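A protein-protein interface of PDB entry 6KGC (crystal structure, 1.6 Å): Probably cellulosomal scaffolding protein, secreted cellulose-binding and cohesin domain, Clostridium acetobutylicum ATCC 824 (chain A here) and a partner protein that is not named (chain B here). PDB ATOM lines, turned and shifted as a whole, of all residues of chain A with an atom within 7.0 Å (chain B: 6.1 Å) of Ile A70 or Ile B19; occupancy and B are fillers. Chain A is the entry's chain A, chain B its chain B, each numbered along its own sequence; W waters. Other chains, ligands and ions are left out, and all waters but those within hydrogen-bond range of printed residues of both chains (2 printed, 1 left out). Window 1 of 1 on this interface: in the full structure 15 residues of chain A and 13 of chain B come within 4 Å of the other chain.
The guanidinium group (NH2) of Arg B23 sits at hydrogen-bond distance from the backbone carbonyl oxygen (O) of Asn A66.
O of Tyr A67 is in hydrogen-bond range of NH2 of Arg B23 (3.1 Å).
The backbone carbonyl oxygen of Val A71 is in hydrogen-bond range of the side-chain hydroxyl of Ser B60 (3.4 Å).
ND2 of Asn A72 lies within hydrogen-bond range of O of Val B59, at 3.0 Å.
NH1 of Arg B23 lies within hydrogen-bond range of OG1 of Thr A84, at 2.6 Å.
O of Tyr A67 sits at hydrogen-bond distance from OG1 of Thr A84 (3.5 Å).
O of Ser A68 lies within hydrogen-bond range of N of Thr A84, at 2.9 Å.
The backbone NH (N) of Ile A70 sits at hydrogen-bond distance from the backbone carbonyl oxygen (O) of Thr A82 (2.9 Å).
The backbone carbonyl oxygen (O) of Ser A80 sits at hydrogen-bond distance from the backbone NH (N) of Asn A72.
OD1 of Asn B15 sits at hydrogen-bond distance from N of Arg B17 (3.1 Å).
CD1 of Leu A37 touches C of Gly B16 (3.9 Å).
CD2 of Leu A37 touches CG of Arg B17 (3.7 Å).
Ile B56 touches Tyr A67 (CD1 to CB, 3.8 Å).
Ile A70 touches Ile B19.
CG2 of Ile B56 touches CD1 of Ile A70, 3.9 Å away.
Ser B60 touches Ile A70 (CB to CG2, 3.7 Å).
Ser B60 touches Asn A72.
OG1 of Thr A82 touches CG1 of Val B59, at 3.9 Å.
Arg B23 touches Leu A88.
Gln B24 touches Leu A88 (CA to CD1, 3.9 Å).
Ile A70 touches just these residues of chain B: Ile B19, Ile B56 and Ser B60.
Of chain A, only Ile A70 comes within 4 Å of Ile B19.
Of the printed residues of chain A, Ile B56 touches Tyr A67 (3.8 Å) and Ile A70 (3.9 Å).
Printed residues of chain A within 4 Å of Ser B60: Ile A70 (3.7 Å), Val A71 (3.4 Å) and Asn A72 (3.4 Å).
Printed residues of chain B within 4 Å of Thr A84: Arg B23.
Phe A83 touches none of the printed residues of chain B.
Asp B18 touches none of the printed residues of chain A.
The nearest residue of chain B that does not touch Ile A70 is Val B59 (4.2 Å).
The nearest residue of chain A that does not touch Ile B19 is Thr A84 (4.6 Å).
Hydrophobic or aromatic side chains of chain B within 4 Å of the printed part of chain A: Ile B19, Ile B56 and Val B59.
Of the 16 printed residues of chain A, 9 touch a printed residue of chain B.
Printed residues of chain A that touch a printed residue of chain B: Leu A37, Asn A66, Tyr A67, Ile A70, Val A71, Asn A72, Thr A82, Thr A84 and Leu A88.
Hydrophobic or aromatic side chains of chain A within 4 Å of the printed part of chain B: Leu A37, Tyr A67, Ile A70 and Leu A88.
Among the printed residues, 16 pairs touch across the chains.
Among the printed residues, no Asp or Glu carboxylate lies within 4 Å of a Lys or Arg side-chain nitrogen of the other chain.
Water W2 bridges the side-chain hydroxyl (OG1) of Thr A82 (2.8 Å) and the backbone NH (N) of Gly B16 (2.9 Å).
Water W1 lies within hydrogen-bond range of NH2 of Arg B23 (2.9 Å) and O of Asn A66 (3.1 Å).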
ATOM      1  N   LEU A  37     -30.622   7.375  12.236  1.00  0.00           N
ATOM      2  CA  LEU A  37     -29.648   8.454  12.200  1.00  0.00           C
ATOM      3  C   LEU A  37     -28.301   7.946  12.681  1.00  0.00           C
ATOM      4  O   LEU A  37     -28.252   7.293  13.726  1.00  0.00           O
ATOM      5  CB  LEU A  37     -30.075   9.642  13.091  1.00  0.00           C
ATOM      6  CG  LEU A  37     -29.095  10.785  13.281  1.00  0.00           C
ATOM      7  CD1 LEU A  37     -28.898  11.498  11.977  1.00  0.00           C
ATOM      8  CD2 LEU A  37     -29.601  11.748  14.358  1.00  0.00           C
ATOM      9  N   ILE A  38     -27.231   8.246  11.934  1.00  0.00           N
ATOM     10  CA  ILE A  38     -25.855   8.035  12.380  1.00  0.00           C
ATOM     11  C   ILE A  38     -25.107   9.328  12.085  1.00  0.00           C
ATOM     12  O   ILE A  38     -25.135   9.815  10.949  1.00  0.00           O
ATOM     13  CB  ILE A  38     -25.164   6.852  11.682  1.00  0.00           C
ATOM     14  CG1 ILE A  38     -25.954   5.560  11.864  1.00  0.00           C
ATOM     15  CG2 ILE A  38     -23.736   6.684  12.266  1.00  0.00           C
ATOM     16  CD1 ILE A  38     -25.518   4.401  10.939  1.00  0.00           C
ATOM     17  N   VAL A  54     -15.634   9.117  -0.141  1.00  0.00           N
ATOM     18  CA  VAL A  54     -16.322   8.309   0.860  1.00  0.00           C
ATOM     19  C   VAL A  54     -17.615   7.808   0.237  1.00  0.00           C
ATOM     20  O   VAL A  54     -18.501   8.617  -0.085  1.00  0.00           O
ATOM     21  CB  VAL A  54     -16.608   9.108   2.140  1.00  0.00           C
ATOM     22  CG1 VAL A  54     -17.363   8.249   3.125  1.00  0.00           C
ATOM     23  CG2 VAL A  54     -15.310   9.664   2.705  1.00  0.00           C
ATOM     24  N   ASN A  66     -31.615  11.095  -2.387  1.00  0.00           N
ATOM     25  CA  ASN A  66     -32.309  12.104  -1.596  1.00  0.00           C
ATOM     26  C   ASN A  66     -31.557  12.390  -0.299  1.00  0.00           C
ATOM     27  O   ASN A  66     -32.161  12.594   0.761  1.00  0.00           O
ATOM     28  CB  ASN A  66     -33.736  11.679  -1.281  1.00  0.00           C
ATOM     29  CG  ASN A  66     -34.614  11.684  -2.494  1.00  0.00           C
ATOM     30  OD1 ASN A  66     -34.811  12.727  -3.119  1.00  0.00           O
ATOM     31  ND2 ASN A  66     -35.147  10.519  -2.850  1.00  0.00           N
ATOM     32  N   TYR A  67     -30.222  12.369  -0.370  1.00  0.00           N
ATOM     33  CA  TYR A  67     -29.357  12.839   0.717  1.00  0.00           C
ATOM     34  C   TYR A  67     -29.511  12.005   1.996  1.00  0.00           C
ATOM     35  O   TYR A  67     -29.480  12.526   3.106  1.00  0.00           O
ATOM     36  CB  TYR A  67     -29.602  14.333   0.974  1.00  0.00           C
ATOM     37  CG  TYR A  67     -29.286  15.176  -0.265  1.00  0.00           C
ATOM     38  CD1 TYR A  67     -27.982  15.500  -0.571  1.00  0.00           C
ATOM     39  CD2 TYR A  67     -30.285  15.593  -1.119  1.00  0.00           C
ATOM     40  CE1 TYR A  67     -27.681  16.241  -1.684  1.00  0.00           C
ATOM     41  CE2 TYR A  67     -29.993  16.325  -2.254  1.00  0.00           C
ATOM     42  CZ  TYR A  67     -28.680  16.640  -2.523  1.00  0.00           C
ATOM     43  OH  TYR A  67     -28.352  17.382  -3.640  1.00  0.00           O
ATOM     44  N   SER A  68     -29.652  10.678   1.834  1.00  0.00           N
ATOM     45  CA  SER A  68     -29.540   9.775   2.970  1.00  0.00           C
ATOM     46  C   SER A  68     -28.118   9.683   3.506  1.00  0.00           C
ATOM     47  O   SER A  68     -27.919   9.198   4.627  1.00  0.00           O
ATOM     48  CB  SER A  68     -30.029   8.378   2.589  1.00  0.00           C
ATOM     49  OG  SER A  68     -29.188   7.831   1.606  1.00  0.00           O
ATOM     50  N   PHE A  69     -27.127  10.140   2.750  1.00  0.00           N
ATOM     51  CA  PHE A  69     -25.713   9.888   3.076  1.00  0.00           C
ATOM     52  C   PHE A  69     -24.944  11.154   2.739  1.00  0.00           C
ATOM     53  O   PHE A  69     -24.712  11.459   1.557  1.00  0.00           O
ATOM     54  CB  PHE A  69     -25.177   8.662   2.291  1.00  0.00           C
ATOM     55  CG  PHE A  69     -23.803   8.188   2.703  1.00  0.00           C
ATOM     56  CD1 PHE A  69     -23.644   7.413   3.826  1.00  0.00           C
ATOM     57  CD2 PHE A  69     -22.694   8.459   1.920  1.00  0.00           C
ATOM     58  CE1 PHE A  69     -22.354   6.962   4.194  1.00  0.00           C
ATOM     59  CE2 PHE A  69     -21.450   8.010   2.278  1.00  0.00           C
ATOM     60  CZ  PHE A  69     -21.299   7.254   3.404  1.00  0.00           C
ATOM     61  N   ILE A  70     -24.523  11.874   3.769  1.00  0.00           N
ATOM     62  CA  ILE A  70     -23.893  13.179   3.622  1.00  0.00           C
ATOM     63  C   ILE A  70     -22.483  13.073   4.168  1.00  0.00           C
ATOM     64  O   ILE A  70     -22.273  12.634   5.303  1.00  0.00           O
ATOM     65  CB  ILE A  70     -24.684  14.286   4.351  1.00  0.00           C
ATOM     66  CG1 ILE A  70     -26.041  14.474   3.699  1.00  0.00           C
ATOM     67  CG2 ILE A  70     -23.935  15.595   4.317  1.00  0.00           C
ATOM     68  CD1 ILE A  70     -27.047  15.150   4.571  1.00  0.00           C
ATOM     69  N   VAL A  71     -21.512  13.475   3.360  1.00  0.00           N
ATOM     70  CA  VAL A  71     -20.118  13.378   3.725  1.00  0.00           C
ATOM     71  C   VAL A  71     -19.523  14.772   3.777  1.00  0.00           C
ATOM     72  O   VAL A  71     -19.692  15.581   2.847  1.00  0.00           O
ATOM     73  CB  VAL A  71     -19.348  12.465   2.748  1.00  0.00           C
ATOM     74  CG1 VAL A  71     -17.874  12.405   3.130  1.00  0.00           C
ATOM     75  CG2 VAL A  71     -19.996  11.098   2.691  1.00  0.00           C
ATOM     76  N   ASN A  72     -18.805  15.045   4.854  1.00  0.00           N
ATOM     77  CA  ASN A  72     -18.103  16.303   5.031  1.00  0.00           C
ATOM     78  C   ASN A  72     -16.616  16.011   5.130  1.00  0.00           C
ATOM     79  O   ASN A  72     -16.144  15.461   6.146  1.00  0.00           O
ATOM     80  CB  ASN A  72     -18.613  17.053   6.269  1.00  0.00           C
ATOM     81  CG  ASN A  72     -17.947  18.415   6.443  1.00  0.00           C
ATOM     82  OD1 ASN A  72     -16.772  18.608   6.131  1.00  0.00           O
ATOM     83  ND2 ASN A  72     -18.708  19.376   6.956  1.00  0.00           N
ATOM     84  N   SER A  80     -16.572  13.477   8.293  1.00  0.00           N
ATOM     85  CA  SER A  80     -17.839  13.393   9.012  1.00  0.00           C
ATOM     86  C   SER A  80     -18.836  12.709   8.092  1.00  0.00           C
ATOM     87  O   SER A  80     -19.014  13.136   6.940  1.00  0.00           O
ATOM     88  CB  SER A  80     -18.358  14.762   9.439  1.00  0.00           C
ATOM     89  OG  SER A  80     -17.448  15.378  10.349  1.00  0.00           O
ATOM     90  N   ILE A  81     -19.457  11.646   8.582  1.00  0.00           N
ATOM     91  CA  ILE A  81     -20.472  10.909   7.854  1.00  0.00           C
ATOM     92  C   ILE A  81     -21.791  11.062   8.585  1.00  0.00           C
ATOM     93  O   ILE A  81     -21.858  10.829   9.809  1.00  0.00           O
ATOM     94  CB  ILE A  81     -20.141   9.411   7.709  1.00  0.00           C
ATOM     95  CG1 ILE A  81     -18.865   9.230   6.900  1.00  0.00           C
ATOM     96  CG2 ILE A  81     -21.314   8.650   7.091  1.00  0.00           C
ATOM     97  CD1 ILE A  81     -18.313   7.812   6.943  1.00  0.00           C
ATOM     98  N   THR A  82     -22.833  11.403   7.836  1.00  0.00           N
ATOM     99  CA  THR A  82     -24.187  11.508   8.347  1.00  0.00           C
ATOM    100  C   THR A  82     -25.101  10.613   7.519  1.00  0.00           C
ATOM    101  O   THR A  82     -25.316  10.856   6.321  1.00  0.00           O
ATOM    102  CB  THR A  82     -24.685  12.960   8.325  1.00  0.00           C
ATOM    103  OG1 THR A  82     -23.770  13.797   9.042  1.00  0.00           O
ATOM    104  CG2 THR A  82     -26.115  13.044   8.944  1.00  0.00           C
ATOM    105  N   PHE A  83     -25.651   9.600   8.165  1.00  0.00           N
ATOM    106  CA  PHE A  83     -26.671   8.750   7.596  1.00  0.00           C
ATOM    107  C   PHE A  83     -28.035   9.133   8.152  1.00  0.00           C
ATOM    108  O   PHE A  83     -28.178   9.311   9.369  1.00  0.00           O
ATOM    109  CB  PHE A  83     -26.434   7.265   7.913  1.00  0.00           C
ATOM    110  CG  PHE A  83     -27.634   6.429   7.652  1.00  0.00           C
ATOM    111  CD1 PHE A  83     -27.968   6.059   6.361  1.00  0.00           C
ATOM    112  CD2 PHE A  83     -28.493   6.071   8.681  1.00  0.00           C
ATOM    113  CE1 PHE A  83     -29.144   5.326   6.106  1.00  0.00           C
ATOM    114  CE2 PHE A  83     -29.669   5.344   8.431  1.00  0.00           C
ATOM    115  CZ  PHE A  83     -29.985   4.964   7.149  1.00  0.00           C
ATOM    116  N   THR A  84     -29.036   9.208   7.258  1.00  0.00           N
ATOM    117  CA  THR A  84     -30.400   9.468   7.662  1.00  0.00           C
ATOM    118  C   THR A  84     -31.337   8.670   6.772  1.00  0.00           C
ATOM    119  O   THR A  84     -30.943   8.132   5.746  1.00  0.00           O
ATOM    120  CB  THR A  84     -30.783  10.960   7.556  1.00  0.00           C
ATOM    121  OG1 THR A  84     -30.547  11.404   6.215  1.00  0.00           O
ATOM    122  CG2 THR A  84     -30.026  11.838   8.524  1.00  0.00           C
ATOM    123  N   LEU A  88     -38.220   8.908   6.787  1.00  0.00           N
ATOM    124  CA  LEU A  88     -38.610   8.888   8.192  1.00  0.00           C
ATOM    125  C   LEU A  88     -39.335   7.600   8.587  1.00  0.00           C
ATOM    126  O   LEU A  88     -40.006   7.559   9.631  1.00  0.00           O
ATOM    127  CB  LEU A  88     -39.471  10.108   8.520  1.00  0.00           C
ATOM    128  CG  LEU A  88     -38.803  11.453   8.218  1.00  0.00           C
ATOM    129  CD1 LEU A  88     -39.856  12.550   8.293  1.00  0.00           C
ATOM    130  CD2 LEU A  88     -37.687  11.698   9.166  1.00  0.00           C
ATOM    131  N   GLY B   6     -30.608  26.800  11.144  1.00  0.00           N
ATOM    132  CA  GLY B   6     -30.325  25.392  10.999  1.00  0.00           C
ATOM    133  C   GLY B   6     -30.187  24.633  12.298  1.00  0.00           C
ATOM    134  O   GLY B   6     -30.231  23.403  12.280  1.00  0.00           O
ATOM    135  N   LEU B   8     -32.192  23.606  14.635  1.00  0.00           N
ATOM    136  CA  LEU B   8     -33.616  23.472  14.929  1.00  0.00           C
ATOM    137  C   LEU B   8     -33.881  23.025  16.363  1.00  0.00           C
ATOM    138  O   LEU B   8     -34.952  23.318  16.909  1.00  0.00           O
ATOM    139  CB  LEU B   8     -34.262  22.496  13.945  1.00  0.00           C
ATOM    140  CG  LEU B   8     -34.646  23.029  12.565  1.00  0.00           C
ATOM    141  CD1 LEU B   8     -33.474  23.649  11.870  1.00  0.00           C
ATOM    142  CD2 LEU B   8     -35.234  21.907  11.690  1.00  0.00           C
ATOM    143  N   ASN B  15     -26.190  19.599  12.831  1.00  0.00           N
ATOM    144  CA  ASN B  15     -25.809  18.249  12.439  1.00  0.00           C
ATOM    145  C   ASN B  15     -27.044  17.488  11.987  1.00  0.00           C
ATOM    146  O   ASN B  15     -28.107  18.069  11.754  1.00  0.00           O
ATOM    147  CB  ASN B  15     -25.082  17.534  13.579  1.00  0.00           C
ATOM    148  CG  ASN B  15     -25.941  17.336  14.821  1.00  0.00           C
ATOM    149  OD1 ASN B  15     -27.154  17.499  14.794  1.00  0.00           O
ATOM    150  ND2 ASN B  15     -25.292  16.980  15.929  1.00  0.00           N
ATOM    151  N   GLY B  16     -26.896  16.173  11.866  1.00  0.00           N
ATOM    152  CA  GLY B  16     -27.947  15.350  11.328  1.00  0.00           C
ATOM    153  C   GLY B  16     -29.241  15.383  12.116  1.00  0.00           C
ATOM    154  O   GLY B  16     -30.316  15.140  11.554  1.00  0.00           O
ATOM    155  N   ARG B  17     -29.166  15.618  13.432  1.00  0.00           N
ATOM    156  CA  ARG B  17     -30.405  15.706  14.203  1.00  0.00           C
ATOM    157  C   ARG B  17     -31.282  16.835  13.682  1.00  0.00           C
ATOM    158  O   ARG B  17     -32.519  16.744  13.706  1.00  0.00           O
ATOM    159  CB  ARG B  17     -30.112  15.942  15.669  1.00  0.00           C
ATOM    160  CG  ARG B  17     -29.380  14.821  16.388  1.00  0.00           C
ATOM    161  CD  ARG B  17     -29.423  15.157  17.860  1.00  0.00           C
ATOM    162  NE  ARG B  17     -28.482  14.478  18.729  1.00  0.00           N
ATOM    163  CZ  ARG B  17     -28.675  13.279  19.270  1.00  0.00           C
ATOM    164  NH1 ARG B  17     -29.750  12.574  18.942  1.00  0.00           N
ATOM    165  NH2 ARG B  17     -27.772  12.776  20.105  1.00  0.00           N
ATOM    166  N   ASP B  18     -30.649  17.927  13.255  1.00  0.00           N
ATOM    167  CA  ASP B  18     -31.384  19.074  12.725  1.00  0.00           C
ATOM    168  C   ASP B  18     -31.997  18.746  11.369  1.00  0.00           C
ATOM    169  O   ASP B  18     -33.112  19.173  11.058  1.00  0.00           O
ATOM    170  CB  ASP B  18     -30.448  20.271  12.618  1.00  0.00           C
ATOM    171  CG  ASP B  18     -29.870  20.688  13.957  1.00  0.00           C
ATOM    172  OD1 ASP B  18     -30.637  21.113  14.829  1.00  0.00           O
ATOM    173  OD2 ASP B  18     -28.641  20.574  14.126  1.00  0.00           O
ATOM    174  N   ILE B  19     -31.288  17.966  10.552  1.00  0.00           N
ATOM    175  CA  ILE B  19     -31.855  17.531   9.284  1.00  0.00           C
ATOM    176  C   ILE B  19     -33.120  16.729   9.522  1.00  0.00           C
ATOM    177  O   ILE B  19     -34.138  16.911   8.840  1.00  0.00           O
ATOM    178  CB  ILE B  19     -30.813  16.719   8.497  1.00  0.00           C
ATOM    179  CG1 ILE B  19     -29.731  17.644   7.974  1.00  0.00           C
ATOM    180  CG2 ILE B  19     -31.464  15.982   7.313  1.00  0.00           C
ATOM    181  CD1 ILE B  19     -28.577  16.908   7.372  1.00  0.00           C
ATOM    182  N   VAL B  20     -33.080  15.817  10.488  1.00  0.00           N
ATOM    183  CA  VAL B  20     -34.241  14.983  10.751  1.00  0.00           C
ATOM    184  C   VAL B  20     -35.428  15.854  11.129  1.00  0.00           C
ATOM    185  O   VAL B  20     -36.562  15.628  10.668  1.00  0.00           O
ATOM    186  CB  VAL B  20     -33.921  13.959  11.857  1.00  0.00           C
ATOM    187  CG1 VAL B  20     -35.187  13.192  12.229  1.00  0.00           C
ATOM    188  CG2 VAL B  20     -32.796  13.043  11.424  1.00  0.00           C
ATOM    189  N   MET B  21     -35.187  16.846  11.998  1.00  0.00           N
ATOM    190  CA  MET B  21     -36.247  17.744  12.447  1.00  0.00           C
ATOM    191  C   MET B  21     -36.819  18.569  11.308  1.00  0.00           C
ATOM    192  O   MET B  21     -38.029  18.786  11.252  1.00  0.00           O
ATOM    193  CB  MET B  21     -35.708  18.651  13.556  1.00  0.00           C
ATOM    194  CG  MET B  21     -35.467  17.916  14.839  1.00  0.00           C
ATOM    195  SD  MET B  21     -34.819  18.996  16.120  1.00  0.00           S
ATOM    196  CE  MET B  21     -36.063  20.259  16.171  1.00  0.00           C
ATOM    197  N   MET B  22     -35.970  19.045  10.388  1.00  0.00           N
ATOM    198  CA  MET B  22     -36.490  19.754   9.219  1.00  0.00           C
ATOM    199  C   MET B  22     -37.372  18.845   8.368  1.00  0.00           C
ATOM    200  O   MET B  22     -38.444  19.255   7.903  1.00  0.00           O
ATOM    201  CB  MET B  22     -35.327  20.300   8.383  1.00  0.00           C
ATOM    202  CG  MET B  22     -35.750  21.026   7.131  1.00  0.00           C
ATOM    203  SD  MET B  22     -36.620  22.572   7.416  1.00  0.00           S
ATOM    204  CE  MET B  22     -35.192  23.655   7.669  1.00  0.00           C
ATOM    205  N   ARG B  23     -36.940  17.607   8.150  1.00  0.00           N
ATOM    206  CA  ARG B  23     -37.730  16.669   7.362  1.00  0.00           C
ATOM    207  C   ARG B  23     -39.069  16.391   8.036  1.00  0.00           C
ATOM    208  O   ARG B  23     -40.111  16.337   7.371  1.00  0.00           O
ATOM    209  CB  ARG B  23     -36.945  15.370   7.141  1.00  0.00           C
ATOM    210  CG  ARG B  23     -35.836  15.534   6.087  1.00  0.00           C
ATOM    211  CD  ARG B  23     -35.125  14.216   5.815  1.00  0.00           C
ATOM    212  NE  ARG B  23     -34.127  14.398   4.779  1.00  0.00           N
ATOM    213  CZ  ARG B  23     -32.959  13.777   4.765  1.00  0.00           C
ATOM    214  NH1 ARG B  23     -32.655  12.940   5.750  1.00  0.00           N
ATOM    215  NH2 ARG B  23     -32.100  14.026   3.800  1.00  0.00           N
ATOM    216  N   GLN B  24     -39.066  16.231   9.366  1.00  0.00           N
ATOM    217  CA  GLN B  24     -40.322  15.983  10.066  1.00  0.00           C
ATOM    218  C   GLN B  24     -41.257  17.172   9.921  1.00  0.00           C
ATOM    219  O   GLN B  24     -42.460  17.003   9.688  1.00  0.00           O
ATOM    220  CB  GLN B  24     -40.066  15.676  11.541  1.00  0.00           C
ATOM    221  CG  GLN B  24     -39.384  14.347  11.784  1.00  0.00           C
ATOM    222  CD  GLN B  24     -38.939  14.192  13.225  1.00  0.00           C
ATOM    223  OE1 GLN B  24     -38.420  15.130  13.829  1.00  0.00           O
ATOM    224  NE2 GLN B  24     -39.130  13.007  13.779  1.00  0.00           N
ATOM    225  N   LEU B  52     -34.257  23.103   3.536  1.00  0.00           N
ATOM    226  CA  LEU B  52     -33.654  21.798   3.780  1.00  0.00           C
ATOM    227  C   LEU B  52     -32.364  21.649   2.988  1.00  0.00           C
ATOM    228  O   LEU B  52     -31.357  21.167   3.508  1.00  0.00           O
ATOM    229  CB  LEU B  52     -34.626  20.676   3.426  1.00  0.00           C
ATOM    230  CG  LEU B  52     -34.088  19.241   3.513  1.00  0.00           C
ATOM    231  CD1 LEU B  52     -33.601  18.899   4.896  1.00  0.00           C
ATOM    232  CD2 LEU B  52     -35.189  18.240   3.058  1.00  0.00           C
ATOM    233  N   LEU B  55     -29.710  23.517   4.663  1.00  0.00           N
ATOM    234  CA  LEU B  55     -29.278  22.840   5.874  1.00  0.00           C
ATOM    235  C   LEU B  55     -28.339  21.687   5.541  1.00  0.00           C
ATOM    236  O   LEU B  55     -27.312  21.491   6.208  1.00  0.00           O
ATOM    237  CB  LEU B  55     -30.511  22.355   6.635  1.00  0.00           C
ATOM    238  CG  LEU B  55     -30.276  21.614   7.946  1.00  0.00           C
ATOM    239  CD1 LEU B  55     -29.487  22.449   8.942  1.00  0.00           C
ATOM    240  CD2 LEU B  55     -31.634  21.187   8.532  1.00  0.00           C
ATOM    241  N   ILE B  56     -28.679  20.902   4.517  1.00  0.00           N
ATOM    242  CA  ILE B  56     -27.816  19.812   4.085  1.00  0.00           C
ATOM    243  C   ILE B  56     -26.461  20.336   3.657  1.00  0.00           C
ATOM    244  O   ILE B  56     -25.431  19.722   3.937  1.00  0.00           O
ATOM    245  CB  ILE B  56     -28.514  19.022   2.963  1.00  0.00           C
ATOM    246  CG1 ILE B  56     -29.642  18.167   3.554  1.00  0.00           C
ATOM    247  CG2 ILE B  56     -27.518  18.158   2.202  1.00  0.00           C
ATOM    248  CD1 ILE B  56     -30.610  17.645   2.520  1.00  0.00           C
ATOM    249  N   VAL B  59     -24.285  21.059   6.707  1.00  0.00           N
ATOM    250  CA  VAL B  59     -23.735  19.838   7.291  1.00  0.00           C
ATOM    251  C   VAL B  59     -22.643  19.271   6.388  1.00  0.00           C
ATOM    252  O   VAL B  59     -21.612  18.766   6.858  1.00  0.00           O
ATOM    253  CB  VAL B  59     -24.866  18.824   7.532  1.00  0.00           C
ATOM    254  CG1 VAL B  59     -24.319  17.496   8.049  1.00  0.00           C
ATOM    255  CG2 VAL B  59     -25.897  19.353   8.523  1.00  0.00           C
ATOM    256  N   SER B  60     -22.833  19.395   5.072  1.00  0.00           N
ATOM    257  CA  SER B  60     -21.935  18.785   4.099  1.00  0.00           C
ATOM    258  C   SER B  60     -20.634  19.556   3.923  1.00  0.00           C
ATOM    259  O   SER B  60     -19.612  18.962   3.539  1.00  0.00           O
ATOM    260  CB  SER B  60     -22.674  18.677   2.752  1.00  0.00           C
ATOM    261  OG  SER B  60     -21.924  17.943   1.796  1.00  0.00           O
HETATM  262  O   HOH W   1     -33.557  15.230   1.590  1.00  0.00           O
HETATM  263  O   HOH W   2     -24.157  15.337  11.354  1.00  0.00           O
